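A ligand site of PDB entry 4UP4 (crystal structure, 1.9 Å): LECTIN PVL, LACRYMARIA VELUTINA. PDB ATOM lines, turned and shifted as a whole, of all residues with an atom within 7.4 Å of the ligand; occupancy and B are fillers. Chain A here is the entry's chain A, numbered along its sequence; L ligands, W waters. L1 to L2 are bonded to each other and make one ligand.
The side-chain amide oxygen (OD1) of Asn 46 lies within hydrogen-bond range of an oxygen (O1) of LG2 L2 (2.6 Å).
N of Glu 79 lies within hydrogen-bond range of O5 of LG2 L2, 2.7 Å away.
N1 of LG2 L2 lies within hydrogen-bond range of O of Gly 52.
NE1 of Trp 54 is in hydrogen-bond range of O1 of LG2 L2 (3.0 Å).
The side-chain amide nitrogen (ND2) of Asn 80 sits at hydrogen-bond distance from an oxygen (O4) of LIG L1 (3.2 Å).
OE1 of Glu 79 sits at hydrogen-bond distance from NE2 of His 59, 2.7 Å away.
The side-chain carboxylate (OE2) of Glu 79 lies within salt-bridge range of the side-chain amino group (NZ) of Lys 58, 2.8 Å away.
O of Glu 79 lies within hydrogen-bond range of N of Ala 107 (2.8 Å).
N of Trp 54 is in hydrogen-bond range of O of Gly 48 (3.0 Å).
N of Arg 55 lies within hydrogen-bond range of ND1 of His 59 (3.1 Å).
The backbone carbonyl oxygen (O) of Gly 76 lies within hydrogen-bond range of the backbone NH (N) of Trp 83.
The backbone NH of Gly 53 lies within hydrogen-bond range of the backbone carbonyl oxygen of Gly 48, 3.4 Å away.
Gly 53 touches the ligand.
His 59 touches the ligand.
Gly 78 touches the ligand.
CZ2 of Trp 83 touches O3 of LG2 L2, 3.7 Å away.
Of the 24 residues printed, 9 come within 4 Å of the ligand.
The nearest printed residue that does not touch the ligand is Phe 47 (4.8 Å).
Water W5 lies within hydrogen-bond range of O2 of LG2 L2 and ND2 of Asn 46.
Water W9 bridges O2 of LIG L1 and O of Gly 52.
Water W7 lies within hydrogen-bond range of the side-chain amide nitrogen (ND2) of Asn 80 (2.9 Å) and an oxygen (O1) of LIG L1 (3.1 Å).
Water W8 bridges OE2 of Glu 79 (3.1 Å) and O1 of LIG L1 (3.3 Å).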
ATOM      1  N   ASN A  45       8.308 -35.683  -4.791  1.00  0.00           N
ATOM      2  CA  ASN A  45       8.558 -36.372  -6.053  1.00  0.00           C
ATOM      3  C   ASN A  45       7.927 -35.585  -7.190  1.00  0.00           C
ATOM      4  O   ASN A  45       7.018 -36.060  -7.899  1.00  0.00           O
ATOM      5  CB  ASN A  45       8.026 -37.803  -5.964  1.00  0.00           C
ATOM      6  CG  ASN A  45       8.460 -38.641  -7.122  1.00  0.00           C
ATOM      7  OD1 ASN A  45       9.607 -38.542  -7.574  1.00  0.00           O
ATOM      8  ND2 ASN A  45       7.538 -39.429  -7.673  1.00  0.00           N
ATOM      9  N   ASN A  46       8.385 -34.351  -7.323  1.00  0.00           N
ATOM     10  CA  ASN A  46       7.858 -33.362  -8.269  1.00  0.00           C
ATOM     11  C   ASN A  46       8.842 -32.174  -8.365  1.00  0.00           C
ATOM     12  O   ASN A  46       9.843 -32.179  -7.676  1.00  0.00           O
ATOM     13  CB  ASN A  46       6.449 -32.919  -7.850  1.00  0.00           C
ATOM     14  CG  ASN A  46       5.505 -32.734  -9.018  1.00  0.00           C
ATOM     15  OD1 ASN A  46       5.788 -32.007  -9.968  1.00  0.00           O
ATOM     16  ND2 ASN A  46       4.373 -33.396  -8.957  1.00  0.00           N
ATOM     17  N   PHE A  47       8.553 -31.205  -9.246  1.00  0.00           N
ATOM     18  CA  PHE A  47       9.407 -30.026  -9.513  1.00  0.00           C
ATOM     19  C   PHE A  47      10.785 -30.424 -10.008  1.00  0.00           C
ATOM     20  O   PHE A  47      11.776 -29.735  -9.733  1.00  0.00           O
ATOM     21  CB  PHE A  47       9.538 -29.117  -8.292  1.00  0.00           C
ATOM     22  CG  PHE A  47       8.209 -28.662  -7.747  1.00  0.00           C
ATOM     23  CD1 PHE A  47       7.511 -27.662  -8.381  1.00  0.00           C
ATOM     24  CD2 PHE A  47       7.658 -29.248  -6.633  1.00  0.00           C
ATOM     25  CE1 PHE A  47       6.285 -27.229  -7.872  1.00  0.00           C
ATOM     26  CE2 PHE A  47       6.446 -28.864  -6.136  1.00  0.00           C
ATOM     27  CZ  PHE A  47       5.748 -27.864  -6.770  1.00  0.00           C
ATOM     28  N   GLY A  48      10.865 -31.568 -10.655  1.00  0.00           N
ATOM     29  CA  GLY A  48      12.145 -32.125 -11.089  1.00  0.00           C
ATOM     30  C   GLY A  48      12.192 -32.321 -12.601  1.00  0.00           C
ATOM     31  O   GLY A  48      11.148 -32.405 -13.255  1.00  0.00           O
ATOM     32  N   ALA A  51      10.808 -35.621 -12.710  1.00  0.00           N
ATOM     33  CA  ALA A  51       9.636 -35.739 -11.869  1.00  0.00           C
ATOM     34  C   ALA A  51       8.737 -34.553 -12.129  1.00  0.00           C
ATOM     35  O   ALA A  51       8.820 -33.522 -11.453  1.00  0.00           O
ATOM     36  CB  ALA A  51      10.064 -35.805 -10.436  1.00  0.00           C
ATOM     37  N   GLY A  52       7.937 -34.660 -13.187  1.00  0.00           N
ATOM     38  CA  GLY A  52       7.140 -33.550 -13.601  1.00  0.00           C
ATOM     39  C   GLY A  52       7.535 -32.810 -14.852  1.00  0.00           C
ATOM     40  O   GLY A  52       6.809 -31.896 -15.287  1.00  0.00           O
ATOM     41  N   GLY A  53       8.654 -33.187 -15.466  1.00  0.00           N
ATOM     42  CA  GLY A  53       9.058 -32.507 -16.693  1.00  0.00           C
ATOM     43  C   GLY A  53       9.458 -31.031 -16.563  1.00  0.00           C
ATOM     44  O   GLY A  53       9.254 -30.221 -17.503  1.00  0.00           O
ATOM     45  N   TRP A  54      10.065 -30.698 -15.419  1.00  0.00           N
ATOM     46  CA  TRP A  54      10.480 -29.320 -15.174  1.00  0.00           C
ATOM     47  C   TRP A  54      11.785 -29.010 -15.932  1.00  0.00           C
ATOM     48  O   TRP A  54      12.731 -29.822 -15.968  1.00  0.00           O
ATOM     49  CB  TRP A  54      10.581 -29.047 -13.676  1.00  0.00           C
ATOM     50  CG  TRP A  54       9.232 -29.050 -13.068  1.00  0.00           C
ATOM     51  CD1 TRP A  54       8.480 -30.152 -12.789  1.00  0.00           C
ATOM     52  CD2 TRP A  54       8.442 -27.916 -12.634  1.00  0.00           C
ATOM     53  NE1 TRP A  54       7.280 -29.789 -12.243  1.00  0.00           N
ATOM     54  CE2 TRP A  54       7.221 -28.431 -12.134  1.00  0.00           C
ATOM     55  CE3 TRP A  54       8.651 -26.531 -12.596  1.00  0.00           C
ATOM     56  CZ2 TRP A  54       6.214 -27.630 -11.630  1.00  0.00           C
ATOM     57  CZ3 TRP A  54       7.640 -25.733 -12.138  1.00  0.00           C
ATOM     58  CH2 TRP A  54       6.433 -26.268 -11.664  1.00  0.00           C
ATOM     59  N   ARG A  55      11.798 -27.842 -16.572  1.00  0.00           N
ATOM     60  CA  ARG A  55      12.851 -27.379 -17.428  1.00  0.00           C
ATOM     61  C   ARG A  55      13.291 -25.958 -17.022  1.00  0.00           C
ATOM     62  O   ARG A  55      12.478 -25.032 -16.883  1.00  0.00           O
ATOM     63  CB  ARG A  55      12.395 -27.372 -18.858  1.00  0.00           C
ATOM     64  CG  ARG A  55      12.008 -28.752 -19.397  1.00  0.00           C
ATOM     65  CD  ARG A  55      13.270 -29.626 -19.539  1.00  0.00           C
ATOM     66  NE  ARG A  55      12.912 -30.899 -20.105  1.00  0.00           N
ATOM     67  CZ  ARG A  55      12.483 -31.930 -19.386  1.00  0.00           C
ATOM     68  NH1 ARG A  55      12.359 -31.853 -18.041  1.00  0.00           N
ATOM     69  NH2 ARG A  55      12.147 -33.038 -20.019  1.00  0.00           N
ATOM     70  N   LYS A  58      12.029 -23.178 -19.354  1.00  0.00           N
ATOM     71  CA  LYS A  58      10.600 -22.902 -19.426  1.00  0.00           C
ATOM     72  C   LYS A  58       9.900 -22.624 -18.160  1.00  0.00           C
ATOM     73  O   LYS A  58       8.821 -22.055 -18.202  1.00  0.00           O
ATOM     74  CB  LYS A  58       9.867 -24.108 -20.090  1.00  0.00           C
ATOM     75  CG  LYS A  58      10.360 -24.439 -21.493  1.00  0.00           C
ATOM     76  CD  LYS A  58       9.534 -25.559 -22.114  1.00  0.00           C
ATOM     77  CE  LYS A  58       8.052 -25.281 -22.155  1.00  0.00           C
ATOM     78  NZ  LYS A  58       7.371 -26.369 -22.914  1.00  0.00           N
ATOM     79  N   HIS A  59      10.441 -23.094 -17.015  1.00  0.00           N
ATOM     80  CA  HIS A  59       9.735 -23.055 -15.738  1.00  0.00           C
ATOM     81  C   HIS A  59      10.599 -22.377 -14.662  1.00  0.00           C
ATOM     82  O   HIS A  59      11.828 -22.247 -14.832  1.00  0.00           O
ATOM     83  CB  HIS A  59       9.379 -24.455 -15.348  1.00  0.00           C
ATOM     84  CG  HIS A  59       8.678 -25.190 -16.424  1.00  0.00           C
ATOM     85  ND1 HIS A  59       9.086 -26.432 -16.874  1.00  0.00           N
ATOM     86  CD2 HIS A  59       7.626 -24.842 -17.192  1.00  0.00           C
ATOM     87  CE1 HIS A  59       8.290 -26.821 -17.863  1.00  0.00           C
ATOM     88  NE2 HIS A  59       7.436 -25.850 -18.098  1.00  0.00           N
ATOM     89  N   GLY A  76       6.389 -23.493  -7.911  1.00  0.00           N
ATOM     90  CA  GLY A  76       6.858 -23.645  -9.264  1.00  0.00           C
ATOM     91  C   GLY A  76       5.876 -23.092 -10.262  1.00  0.00           C
ATOM     92  O   GLY A  76       4.677 -23.409 -10.229  1.00  0.00           O
ATOM     93  N   PHE A  77       6.399 -22.213 -11.111  1.00  0.00           N
ATOM     94  CA  PHE A  77       5.733 -21.712 -12.279  1.00  0.00           C
ATOM     95  C   PHE A  77       5.941 -22.688 -13.423  1.00  0.00           C
ATOM     96  O   PHE A  77       6.980 -22.696 -14.080  1.00  0.00           O
ATOM     97  CB  PHE A  77       6.301 -20.343 -12.639  1.00  0.00           C
ATOM     98  CG  PHE A  77       6.109 -19.310 -11.558  1.00  0.00           C
ATOM     99  CD1 PHE A  77       7.048 -19.145 -10.519  1.00  0.00           C
ATOM    100  CD2 PHE A  77       5.027 -18.447 -11.595  1.00  0.00           C
ATOM    101  CE1 PHE A  77       6.852 -18.192  -9.524  1.00  0.00           C
ATOM    102  CE2 PHE A  77       4.879 -17.449 -10.624  1.00  0.00           C
ATOM    103  CZ  PHE A  77       5.762 -17.350  -9.582  1.00  0.00           C
ATOM    104  N   GLY A  78       4.966 -23.551 -13.620  1.00  0.00           N
ATOM    105  CA  GLY A  78       5.137 -24.666 -14.514  1.00  0.00           C
ATOM    106  C   GLY A  78       4.591 -24.425 -15.892  1.00  0.00           C
ATOM    107  O   GLY A  78       4.605 -23.336 -16.408  1.00  0.00           O
ATOM    108  N   GLU A  79       4.070 -25.478 -16.521  1.00  0.00           N
ATOM    109  CA  GLU A  79       3.626 -25.385 -17.935  1.00  0.00           C
ATOM    110  C   GLU A  79       2.298 -24.700 -18.070  1.00  0.00           C
ATOM    111  O   GLU A  79       2.127 -23.840 -18.920  1.00  0.00           O
ATOM    112  CB  GLU A  79       3.531 -26.768 -18.570  1.00  0.00           C
ATOM    113  CG  GLU A  79       3.401 -26.779 -20.091  1.00  0.00           C
ATOM    114  CD  GLU A  79       4.693 -26.403 -20.804  1.00  0.00           C
ATOM    115  OE1 GLU A  79       5.737 -26.085 -20.151  1.00  0.00           O
ATOM    116  OE2 GLU A  79       4.670 -26.316 -22.036  1.00  0.00           O
ATOM    117  N   ASN A  80       1.319 -25.106 -17.262  1.00  0.00           N
ATOM    118  CA  ASN A  80      -0.051 -24.596 -17.336  1.00  0.00           C
ATOM    119  C   ASN A  80      -0.578 -23.883 -16.125  1.00  0.00           C
ATOM    120  O   ASN A  80      -1.715 -23.568 -16.052  1.00  0.00           O
ATOM    121  CB  ASN A  80      -1.003 -25.750 -17.706  1.00  0.00           C
ATOM    122  CG  ASN A  80      -0.719 -26.202 -19.095  1.00  0.00           C
ATOM    123  OD1 ASN A  80      -1.029 -25.493 -19.997  1.00  0.00           O
ATOM    124  ND2 ASN A  80       0.006 -27.283 -19.259  1.00  0.00           N
ATOM    125  N   GLY A  81       0.302 -23.573 -15.197  1.00  0.00           N
ATOM    126  CA  GLY A  81      -0.094 -22.818 -14.034  1.00  0.00           C
ATOM    127  C   GLY A  81       0.951 -22.825 -12.969  1.00  0.00           C
ATOM    128  O   GLY A  81       2.107 -23.345 -13.165  1.00  0.00           O
ATOM    129  N   VAL A  82       0.559 -22.292 -11.823  1.00  0.00           N
ATOM    130  CA  VAL A  82       1.450 -22.186 -10.671  1.00  0.00           C
ATOM    131  C   VAL A  82       1.115 -23.324  -9.719  1.00  0.00           C
ATOM    132  O   VAL A  82      -0.049 -23.487  -9.303  1.00  0.00           O
ATOM    133  CB  VAL A  82       1.307 -20.829  -9.957  1.00  0.00           C
ATOM    134  CG1 VAL A  82       2.142 -20.750  -8.684  1.00  0.00           C
ATOM    135  CG2 VAL A  82       1.700 -19.712 -10.903  1.00  0.00           C
ATOM    136  N   TRP A  83       2.132 -24.086  -9.360  1.00  0.00           N
ATOM    137  CA  TRP A  83       2.005 -25.249  -8.489  1.00  0.00           C
ATOM    138  C   TRP A  83       2.702 -25.060  -7.120  1.00  0.00           C
ATOM    139  O   TRP A  83       3.858 -24.653  -7.090  1.00  0.00           O
ATOM    140  CB  TRP A  83       2.615 -26.443  -9.151  1.00  0.00           C
ATOM    141  CG  TRP A  83       1.913 -26.897 -10.371  1.00  0.00           C
ATOM    142  CD1 TRP A  83       2.120 -26.476 -11.632  1.00  0.00           C
ATOM    143  CD2 TRP A  83       0.927 -27.945 -10.452  1.00  0.00           C
ATOM    144  NE1 TRP A  83       1.321 -27.183 -12.502  1.00  0.00           N
ATOM    145  CE2 TRP A  83       0.595 -28.102 -11.793  1.00  0.00           C
ATOM    146  CE3 TRP A  83       0.301 -28.789  -9.493  1.00  0.00           C
ATOM    147  CZ2 TRP A  83      -0.369 -29.046 -12.232  1.00  0.00           C
ATOM    148  CZ3 TRP A  83      -0.668 -29.739  -9.937  1.00  0.00           C
ATOM    149  CH2 TRP A  83      -0.986 -29.841 -11.282  1.00  0.00           C
ATOM    150  N   PRO A  96       1.170 -34.735  -3.792  1.00  0.00           N
ATOM    151  CA  PRO A  96       1.610 -33.827  -4.812  1.00  0.00           C
ATOM    152  C   PRO A  96       1.328 -32.358  -4.509  1.00  0.00           C
ATOM    153  O   PRO A  96       0.464 -32.036  -3.661  1.00  0.00           O
ATOM    154  CB  PRO A  96       0.807 -34.279  -6.063  1.00  0.00           C
ATOM    155  CG  PRO A  96      -0.446 -34.852  -5.484  1.00  0.00           C
ATOM    156  CD  PRO A  96       0.010 -35.533  -4.231  1.00  0.00           C
ATOM    157  N   PRO A  97       1.977 -31.474  -5.250  1.00  0.00           N
ATOM    158  CA  PRO A  97       1.599 -30.097  -5.201  1.00  0.00           C
ATOM    159  C   PRO A  97       0.219 -29.815  -5.759  1.00  0.00           C
ATOM    160  O   PRO A  97      -0.324 -30.582  -6.552  1.00  0.00           O
ATOM    161  CB  PRO A  97       2.636 -29.419  -6.074  1.00  0.00           C
ATOM    162  CG  PRO A  97       3.007 -30.476  -7.063  1.00  0.00           C
ATOM    163  CD  PRO A  97       3.002 -31.743  -6.278  1.00  0.00           C
ATOM    164  N   MET A  99      -2.287 -27.054  -7.963  1.00  0.00           N
ATOM    165  CA  MET A  99      -2.332 -25.990  -8.969  1.00  0.00           C
ATOM    166  C   MET A  99      -3.264 -24.830  -8.484  1.00  0.00           C
ATOM    167  O   MET A  99      -4.480 -24.948  -8.501  1.00  0.00           O
ATOM    168  CB  MET A  99      -2.800 -26.602 -10.302  1.00  0.00           C
ATOM    169  CG  MET A  99      -2.203 -25.853 -11.522  1.00  0.00           C
ATOM    170  SD  MET A  99      -2.899 -24.200 -11.704  1.00  0.00           S
ATOM    171  CE  MET A  99      -4.581 -24.626 -12.200  1.00  0.00           C
ATOM    172  N   ALA A 105       2.485 -18.779 -16.497  1.00  0.00           N
ATOM    173  CA  ALA A 105       3.008 -20.031 -16.973  1.00  0.00           C
ATOM    174  C   ALA A 105       3.267 -20.017 -18.480  1.00  0.00           C
ATOM    175  O   ALA A 105       2.741 -19.212 -19.250  1.00  0.00           O
ATOM    176  CB  ALA A 105       2.099 -21.187 -16.607  1.00  0.00           C
ATOM    177  N   ALA A 107       2.354 -21.869 -20.964  1.00  0.00           N
ATOM    178  CA  ALA A 107       1.260 -22.124 -21.895  1.00  0.00           C
ATOM    179  C   ALA A 107      -0.024 -21.561 -21.230  1.00  0.00           C
ATOM    180  O   ALA A 107      -1.138 -21.765 -21.696  1.00  0.00           O
ATOM    181  CB  ALA A 107       1.148 -23.601 -22.208  1.00  0.00           C
HETATM  182  C1  LIG L   1       1.817 -30.925 -19.716  1.00  0.00           C
HETATM  183  C2  LIG L   1       2.407 -30.292 -18.452  1.00  0.00           C
HETATM  184  C3  LIG L   1       1.785 -30.879 -17.215  1.00  0.00           C
HETATM  185  C4  LIG L   1       0.287 -30.630 -17.208  1.00  0.00           C
HETATM  186  C5  LIG L   1      -0.287 -31.071 -18.583  1.00  0.00           C
HETATM  187  C6  LIG L   1      -1.683 -30.513 -18.868  1.00  0.00           C
HETATM  188  O1  LIG L   1       2.347 -30.220 -20.785  1.00  0.00           O
HETATM  189  O2  LIG L   1       3.769 -30.608 -18.450  1.00  0.00           O
HETATM  190  O3  LIG L   1       2.357 -30.238 -16.087  1.00  0.00           O
HETATM  191  O4  LIG L   1      -0.092 -29.309 -16.769  1.00  0.00           O
HETATM  192  O5  LIG L   1       0.459 -30.676 -19.716  1.00  0.00           O
HETATM  193  O6  LIG L   1      -2.252 -31.364 -19.864  1.00  0.00           O
HETATM  194  C1  LG2 L   2       2.604 -31.144 -15.007  1.00  0.00           C
HETATM  195  C2  LG2 L   2       3.497 -30.403 -13.976  1.00  0.00           C
HETATM  196  C3  LG2 L   2       3.750 -31.298 -12.751  1.00  0.00           C
HETATM  197  C4  LG2 L   2       2.448 -31.899 -12.219  1.00  0.00           C
HETATM  198  C5  LG2 L   2       1.658 -32.516 -13.382  1.00  0.00           C
HETATM  199  C6  LG2 L   2       0.297 -33.027 -12.916  1.00  0.00           C
HETATM  200  C7  LG2 L   2       4.968 -28.733 -15.057  1.00  0.00           C
HETATM  201  C8  LG2 L   2       6.351 -28.531 -15.549  1.00  0.00           C
HETATM  202  N1  LG2 L   2       4.742 -29.955 -14.584  1.00  0.00           N
HETATM  203  O1  LG2 L   2       4.428 -30.604 -11.713  1.00  0.00           O
HETATM  204  O2  LG2 L   2       2.706 -32.922 -11.283  1.00  0.00           O
HETATM  205  O3  LG2 L   2       1.405 -31.551 -14.382  1.00  0.00           O
HETATM  206  O4  LG2 L   2      -0.328 -33.694 -13.999  1.00  0.00           O
HETATM  207  O5  LG2 L   2       4.125 -27.807 -15.089  1.00  0.00           O
HETATM  208  O   HOH W   1      -0.277 -32.456 -21.660  1.00  0.00           O
HETATM  209  O   HOH W   2      -3.971 -30.315 -22.228  1.00  0.00           O
HETATM  210  O   HOH W   3      -3.087 -34.145 -20.934  1.00  0.00           O
HETATM  211  O   HOH W   4       1.480 -27.499 -15.478  1.00  0.00           O
HETATM  212  O   HOH W   5       4.078 -34.951 -11.852  1.00  0.00           O
HETATM  213  O   HOH W   6       0.620 -33.194  -9.229  1.00  0.00           O
HETATM  214  O   HOH W   7       0.379 -28.103 -22.000  1.00  0.00           O
HETATM  215  O   HOH W   8       4.773 -29.342 -22.782  1.00  0.00           O
HETATM  216  O   HOH W   9       5.042 -32.628 -17.620  1.00  0.00           O
